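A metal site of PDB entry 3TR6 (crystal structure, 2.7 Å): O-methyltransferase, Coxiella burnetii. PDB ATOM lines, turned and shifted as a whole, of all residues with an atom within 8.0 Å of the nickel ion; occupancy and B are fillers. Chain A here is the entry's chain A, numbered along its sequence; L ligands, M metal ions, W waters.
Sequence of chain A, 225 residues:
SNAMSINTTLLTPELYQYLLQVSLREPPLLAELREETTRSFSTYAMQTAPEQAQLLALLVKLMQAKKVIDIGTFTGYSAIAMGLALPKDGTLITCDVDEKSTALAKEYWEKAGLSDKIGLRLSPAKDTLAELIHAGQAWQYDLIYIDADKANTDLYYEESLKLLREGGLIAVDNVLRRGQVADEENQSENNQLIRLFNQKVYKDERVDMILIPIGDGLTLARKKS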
ATOM      1  N   ALA A  45      -9.158   0.906  15.449  1.00  0.00           N
ATOM      2  CA  ALA A  45      -9.260  -0.315  14.653  1.00  0.00           C
ATOM      3  C   ALA A  45     -10.608  -0.483  13.933  1.00  0.00           C
ATOM      4  O   ALA A  45     -10.686  -1.161  12.908  1.00  0.00           O
ATOM      5  CB  ALA A  45      -8.961  -1.538  15.503  1.00  0.00           C
ATOM      6  N   MET A  46     -11.664   0.121  14.464  1.00  0.00           N
ATOM      7  CA  MET A  46     -12.971   0.029  13.820  1.00  0.00           C
ATOM      8  C   MET A  46     -13.054   0.912  12.573  1.00  0.00           C
ATOM      9  O   MET A  46     -14.114   1.038  11.957  1.00  0.00           O
ATOM     10  CB  MET A  46     -14.109   0.330  14.809  1.00  0.00           C
ATOM     11  CG  MET A  46     -14.003   1.656  15.549  1.00  0.00           C
ATOM     12  SD  MET A  46     -15.410   1.883  16.906  1.00  0.00           S
ATOM     13  CE  MET A  46     -16.154   0.084  16.871  1.00  0.00           C
ATOM     14  N   GLN A  47     -11.932   1.503  12.188  1.00  0.00           N
ATOM     15  CA  GLN A  47     -11.867   2.307  10.982  1.00  0.00           C
ATOM     16  C   GLN A  47     -11.959   1.444   9.733  1.00  0.00           C
ATOM     17  O   GLN A  47     -11.474   0.308   9.702  1.00  0.00           O
ATOM     18  CB  GLN A  47     -10.587   3.140  10.956  1.00  0.00           C
ATOM     19  CG  GLN A  47     -10.554   4.211   9.878  1.00  0.00           C
ATOM     20  CD  GLN A  47      -9.284   5.041   9.929  1.00  0.00           C
ATOM     21  OE1 GLN A  47      -8.227   4.557  10.326  1.00  0.00           O
ATOM     22  NE2 GLN A  47      -9.389   6.302   9.535  1.00  0.00           N
ATOM     23  N   THR A  48     -12.595   1.978   8.689  1.00  0.00           N
ATOM     24  CA  THR A  48     -12.773   1.237   7.449  1.00  0.00           C
ATOM     25  C   THR A  48     -11.428   0.968   6.786  1.00  0.00           C
ATOM     26  O   THR A  48     -10.578   1.864   6.699  1.00  0.00           O
ATOM     27  CB  THR A  48     -13.697   1.998   6.477  1.00  0.00           C
ATOM     28  OG1 THR A  48     -14.988   2.165   7.072  1.00  0.00           O
ATOM     29  CG2 THR A  48     -13.853   1.239   5.172  1.00  0.00           C
ATOM     30  N   ALA A  49     -11.248  -0.255   6.317  1.00  0.00           N
ATOM     31  CA  ALA A  49     -10.037  -0.642   5.604  1.00  0.00           C
ATOM     32  C   ALA A  49      -9.880   0.196   4.328  1.00  0.00           C
ATOM     33  O   ALA A  49     -10.846   0.364   3.581  1.00  0.00           O
ATOM     34  CB  ALA A  49     -10.050  -2.122   5.266  1.00  0.00           C
ATOM     35  N   GLN A  52     -11.218  -1.509   1.306  1.00  0.00           N
ATOM     36  CA  GLN A  52     -12.664  -1.666   1.280  1.00  0.00           C
ATOM     37  C   GLN A  52     -13.330  -0.339   0.911  1.00  0.00           C
ATOM     38  O   GLN A  52     -14.276  -0.301   0.124  1.00  0.00           O
ATOM     39  CB  GLN A  52     -13.199  -2.169   2.617  1.00  0.00           C
ATOM     40  CG  GLN A  52     -14.664  -2.592   2.554  1.00  0.00           C
ATOM     41  CD  GLN A  52     -15.264  -2.880   3.914  1.00  0.00           C
ATOM     42  OE1 GLN A  52     -15.687  -1.975   4.625  1.00  0.00           O
ATOM     43  NE2 GLN A  52     -15.317  -4.165   4.272  1.00  0.00           N
ATOM     44  N   ILE A  71     -23.706   5.191   7.513  1.00  0.00           N
ATOM     45  CA  ILE A  71     -24.057   4.865   8.894  1.00  0.00           C
ATOM     46  C   ILE A  71     -22.832   4.442   9.716  1.00  0.00           C
ATOM     47  O   ILE A  71     -22.306   3.342   9.542  1.00  0.00           O
ATOM     48  CB  ILE A  71     -25.127   3.763   8.952  1.00  0.00           C
ATOM     49  CG1 ILE A  71     -26.336   4.157   8.113  1.00  0.00           C
ATOM     50  CG2 ILE A  71     -25.535   3.508  10.397  1.00  0.00           C
ATOM     51  CD1 ILE A  71     -27.468   3.147   8.167  1.00  0.00           C
ATOM     52  N   GLY A  72     -22.401   5.320  10.616  1.00  0.00           N
ATOM     53  CA  GLY A  72     -21.210   5.083  11.416  1.00  0.00           C
ATOM     54  C   GLY A  72     -20.042   5.920  10.948  1.00  0.00           C
ATOM     55  O   GLY A  72     -19.182   5.441  10.207  1.00  0.00           O
ATOM     56  N   SER A  78     -14.844   6.476   5.641  1.00  0.00           N
ATOM     57  CA  SER A  78     -15.723   5.999   4.581  1.00  0.00           C
ATOM     58  C   SER A  78     -16.582   7.123   4.010  1.00  0.00           C
ATOM     59  O   SER A  78     -16.886   7.150   2.823  1.00  0.00           O
ATOM     60  CB  SER A  78     -16.612   4.864   5.090  1.00  0.00           C
ATOM     61  OG  SER A  78     -17.367   5.257   6.216  1.00  0.00           O
ATOM     62  N   TYR A 145     -24.285   2.651   3.270  1.00  0.00           N
ATOM     63  CA  TYR A 145     -23.202   1.892   3.878  1.00  0.00           C
ATOM     64  C   TYR A 145     -23.435   1.755   5.382  1.00  0.00           C
ATOM     65  O   TYR A 145     -23.412   2.743   6.112  1.00  0.00           O
ATOM     66  CB  TYR A 145     -21.865   2.586   3.599  1.00  0.00           C
ATOM     67  CG  TYR A 145     -20.654   1.922   4.239  1.00  0.00           C
ATOM     68  CD1 TYR A 145     -20.384   0.575   4.043  1.00  0.00           C
ATOM     69  CD2 TYR A 145     -19.765   2.669   5.002  1.00  0.00           C
ATOM     70  CE1 TYR A 145     -19.267  -0.020   4.624  1.00  0.00           C
ATOM     71  CE2 TYR A 145     -18.653   2.085   5.577  1.00  0.00           C
ATOM     72  CZ  TYR A 145     -18.396   0.744   5.385  1.00  0.00           C
ATOM     73  OH  TYR A 145     -17.286   0.172   5.966  1.00  0.00           O
ATOM     74  N   ILE A 146     -23.654   0.525   5.826  1.00  0.00           N
ATOM     75  CA  ILE A 146     -23.969   0.244   7.221  1.00  0.00           C
ATOM     76  C   ILE A 146     -22.740  -0.224   7.978  1.00  0.00           C
ATOM     77  O   ILE A 146     -22.244  -1.325   7.755  1.00  0.00           O
ATOM     78  CB  ILE A 146     -25.054  -0.833   7.333  1.00  0.00           C
ATOM     79  CG1 ILE A 146     -26.317  -0.419   6.577  1.00  0.00           C
ATOM     80  CG2 ILE A 146     -25.344  -1.129   8.804  1.00  0.00           C
ATOM     81  CD1 ILE A 146     -27.362  -1.494   6.475  1.00  0.00           C
ATOM     82  N   ASP A 147     -22.262   0.612   8.904  1.00  0.00           N
ATOM     83  CA  ASP A 147     -21.026   0.327   9.627  1.00  0.00           C
ATOM     84  C   ASP A 147     -21.011   0.994  11.009  1.00  0.00           C
ATOM     85  O   ASP A 147     -20.073   1.722  11.348  1.00  0.00           O
ATOM     86  CB  ASP A 147     -19.819   0.742   8.782  1.00  0.00           C
ATOM     87  CG  ASP A 147     -18.503   0.341   9.409  1.00  0.00           C
ATOM     88  OD1 ASP A 147     -17.457   0.870   8.971  1.00  0.00           O
ATOM     89  OD2 ASP A 147     -18.519  -0.488  10.332  1.00  0.00           O
ATOM     90  N   ALA A 148     -22.049   0.751  11.798  1.00  0.00           N
ATOM     91  CA  ALA A 148     -22.140   1.305  13.142  1.00  0.00           C
ATOM     92  C   ALA A 148     -22.234   0.194  14.191  1.00  0.00           C
ATOM     93  O   ALA A 148     -21.552  -0.825  14.078  1.00  0.00           O
ATOM     94  CB  ALA A 148     -23.345   2.234  13.244  1.00  0.00           C
ATOM     95  N   LYS A 150     -23.176  -3.023  15.779  1.00  0.00           N
ATOM     96  CA  LYS A 150     -23.536  -4.265  15.084  1.00  0.00           C
ATOM     97  C   LYS A 150     -24.860  -4.864  15.558  1.00  0.00           C
ATOM     98  O   LYS A 150     -25.516  -5.591  14.822  1.00  0.00           O
ATOM     99  CB  LYS A 150     -22.413  -5.299  15.196  1.00  0.00           C
ATOM    100  CG  LYS A 150     -21.033  -4.761  14.829  1.00  0.00           C
ATOM    101  CD  LYS A 150     -21.035  -4.036  13.488  1.00  0.00           C
ATOM    102  CE  LYS A 150     -19.677  -3.399  13.216  1.00  0.00           C
ATOM    103  NZ  LYS A 150     -19.716  -2.384  12.122  1.00  0.00           N
ATOM    104  N   VAL A 172     -22.747  -3.676   3.626  1.00  0.00           N
ATOM    105  CA  VAL A 172     -22.614  -3.980   5.043  1.00  0.00           C
ATOM    106  C   VAL A 172     -21.215  -4.485   5.361  1.00  0.00           C
ATOM    107  O   VAL A 172     -20.739  -5.448   4.766  1.00  0.00           O
ATOM    108  CB  VAL A 172     -23.650  -5.041   5.489  1.00  0.00           C
ATOM    109  CG1 VAL A 172     -23.532  -5.304   6.989  1.00  0.00           C
ATOM    110  CG2 VAL A 172     -25.061  -4.581   5.134  1.00  0.00           C
ATOM    111  N   ASP A 173     -20.552  -3.827   6.310  1.00  0.00           N
ATOM    112  CA  ASP A 173     -19.211  -4.214   6.711  1.00  0.00           C
ATOM    113  C   ASP A 173     -19.244  -5.205   7.878  1.00  0.00           C
ATOM    114  O   ASP A 173     -20.268  -5.357   8.551  1.00  0.00           O
ATOM    115  CB  ASP A 173     -18.399  -2.974   7.097  1.00  0.00           C
ATOM    116  CG  ASP A 173     -16.922  -3.279   7.305  1.00  0.00           C
ATOM    117  OD1 ASP A 173     -16.474  -4.393   6.933  1.00  0.00           O
ATOM    118  OD2 ASP A 173     -16.206  -2.399   7.821  1.00  0.00           O
ATOM    119  N   ASN A 174     -18.117  -5.879   8.106  1.00  0.00           N
ATOM    120  CA  ASN A 174     -17.928  -6.746   9.272  1.00  0.00           C
ATOM    121  C   ASN A 174     -18.838  -7.968   9.334  1.00  0.00           C
ATOM    122  O   ASN A 174     -19.186  -8.436  10.414  1.00  0.00           O
ATOM    123  CB  ASN A 174     -18.053  -5.945  10.575  1.00  0.00           C
ATOM    124  CG  ASN A 174     -17.101  -4.766  10.630  1.00  0.00           C
ATOM    125  OD1 ASN A 174     -15.884  -4.925  10.811  1.00  0.00           O
ATOM    126  ND2 ASN A 174     -17.646  -3.561  10.480  1.00  0.00           N
ATOM    127  N   VAL A 175     -19.215  -8.498   8.169  1.00  0.00           N
ATOM    128  CA  VAL A 175     -20.067  -9.685   8.119  1.00  0.00           C
ATOM    129  C   VAL A 175     -19.288 -10.980   8.382  1.00  0.00           C
ATOM    130  O   VAL A 175     -19.887 -12.036   8.589  1.00  0.00           O
ATOM    131  CB  VAL A 175     -20.809  -9.801   6.774  1.00  0.00           C
ATOM    132  CG1 VAL A 175     -21.923  -8.764   6.688  1.00  0.00           C
ATOM    133  CG2 VAL A 175     -19.847  -9.659   5.607  1.00  0.00           C
ATOM    134  N   GLY A 215     -11.728  -6.091   3.253  1.00  0.00           N
ATOM    135  CA  GLY A 215     -11.925  -5.578   4.604  1.00  0.00           C
ATOM    136  C   GLY A 215     -12.355  -6.737   5.490  1.00  0.00           C
ATOM    137  O   GLY A 215     -11.892  -7.861   5.316  1.00  0.00           O
ATOM    138  N   ASP A 216     -13.266  -6.480   6.432  1.00  0.00           N
ATOM    139  CA  ASP A 216     -13.784  -7.546   7.277  1.00  0.00           C
ATOM    140  C   ASP A 216     -14.995  -8.228   6.634  1.00  0.00           C
ATOM    141  O   ASP A 216     -15.879  -8.748   7.325  1.00  0.00           O
ATOM    142  CB  ASP A 216     -14.137  -7.023   8.664  1.00  0.00           C
ATOM    143  CG  ASP A 216     -14.421  -8.141   9.655  1.00  0.00           C
ATOM    144  OD1 ASP A 216     -13.701  -9.157   9.620  1.00  0.00           O
ATOM    145  OD2 ASP A 216     -15.362  -7.995  10.468  1.00  0.00           O
ATOM    146  N   GLY A 217     -15.027  -8.235   5.303  1.00  0.00           N
ATOM    147  CA  GLY A 217     -16.160  -8.784   4.585  1.00  0.00           C
ATOM    148  C   GLY A 217     -17.159  -7.698   4.271  1.00  0.00           C
ATOM    149  O   GLY A 217     -17.567  -6.935   5.153  1.00  0.00           O
HETATM  150  N1  LIG L   1     -17.259   3.815   8.654  1.00  0.00           N
HETATM  151  C1  LIG L   1     -16.481   4.260   9.779  1.00  0.00           C
HETATM  152  C2  LIG L   1     -16.478   3.238  10.893  1.00  0.00           C
HETATM  153  C3  LIG L   1     -17.242   3.606  12.150  1.00  0.00           C
HETATM  154  S1  LIG L   1     -17.082   2.518  13.562  1.00  0.00           S
HETATM  155  C4  LIG L   1     -15.082   4.527   9.348  1.00  0.00           C
HETATM  156  O1  LIG L   1     -14.166   4.576  10.219  1.00  0.00           O
HETATM  157  O2  LIG L   1     -14.795   4.691   8.130  1.00  0.00           O
HETATM  158  C5  LIG L   1     -18.591   2.530  14.510  1.00  0.00           C
HETATM  159  C6  LIG L   1     -19.187   3.804  14.766  1.00  0.00           C
HETATM  160  O3  LIG L   1     -20.623   3.626  15.044  1.00  0.00           O
HETATM  161  C7  LIG L   1     -18.603   4.428  15.967  1.00  0.00           C
HETATM  162  O4  LIG L   1     -18.089   5.655  15.637  1.00  0.00           O
HETATM  163  C8  LIG L   1     -19.719   4.586  16.909  1.00  0.00           C
HETATM  164  O5  LIG L   1     -19.634   5.778  17.579  1.00  0.00           O
HETATM  165  C9  LIG L   1     -20.912   4.575  16.028  1.00  0.00           C
HETATM  166  N2  LIG L   1     -22.194   4.249  16.665  1.00  0.00           N
HETATM  167  C10 LIG L   1     -22.395   3.370  17.652  1.00  0.00           C
HETATM  168  N3  LIG L   1     -23.710   3.370  17.942  1.00  0.00           N
HETATM  169  C11 LIG L   1     -24.333   4.253  17.138  1.00  0.00           C
HETATM  170  C12 LIG L   1     -25.658   4.672  16.990  1.00  0.00           C
HETATM  171  N4  LIG L   1     -26.694   4.117  17.815  1.00  0.00           N
HETATM  172  N5  LIG L   1     -25.956   5.593  16.055  1.00  0.00           N
HETATM  173  C13 LIG L   1     -25.001   6.118  15.282  1.00  0.00           C
HETATM  174  N6  LIG L   1     -23.720   5.749  15.402  1.00  0.00           N
HETATM  175  C14 LIG L   1     -23.364   4.817  16.312  1.00  0.00           C
HETATM  176 NI    NI M   1     -16.166  -1.536  10.176  1.00  0.00          NI
HETATM  177  O   HOH W   1     -17.060  -0.914  12.928  1.00  0.00           O
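N1 of the ligand lies within salt-bridge range of OD1 of Asp 147, 3.0 Å away. N of Thr 48 lies within hydrogen-bond range of O1 of the ligand (3.4 Å). The side-chain hydroxyl (OG1) of Thr 48 lies within hydrogen-bond range of an oxygen (O2) of the ligand. O of Gly 72 sits at hydrogen-bond distance from N1 of the ligand (3.0 Å). N of Ser 78 sits at hydrogen-bond distance from O2 of the ligand. OG of Ser 78 sits at hydrogen-bond distance from N1 of the ligand, 2.8 Å away.
Water W1 lies within hydrogen-bond range of the side-chain amino group (NZ) of Lys 150 and a sulfur (S1) of the ligand.
OD2 of Asp 173 lies close to OH of Tyr 145, 3.3 Å away. The side-chain carboxylate (OD1) of Asp 173 is in hydrogen-bond range of the side-chain amide nitrogen (NE2) of Gln 52, at 2.9 Å. N of Asp 173 is in hydrogen-bond range of O of Ile 146 (3.3 Å). ND2 of Asn 174 lies close to NZ of Lys 150, 2.9 Å away. OD1 of Asn 174 sits close to OD2 of Asp 216 (3.1 Å). The backbone NH (N) of Asn 174 is in hydrogen-bond range of the backbone carbonyl oxygen (O) of Gly 217 (3.2 Å). The side-chain carboxylate of Asp 147 lies close to the side-chain amino group of Lys 150. N of Asp 147 is in hydrogen-bond range of O of Ile 71, 2.8 Å away.
Met 46 touches the nickel ion. Within 4 Å of the nickel ion: Met 46, Asp 147, Asp 173 and Asn 174. The nearest printed residue that does not touch the nickel ion is Lys 150 (4.1 Å).
The nickel ion is bound by OD2 of Asp 173 (2.5 Å), ND2 of Asn 174 (2.5 Å) and OD2 of Asp 147 (2.6 Å). The nickel ion has three donor atoms within binding distance.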
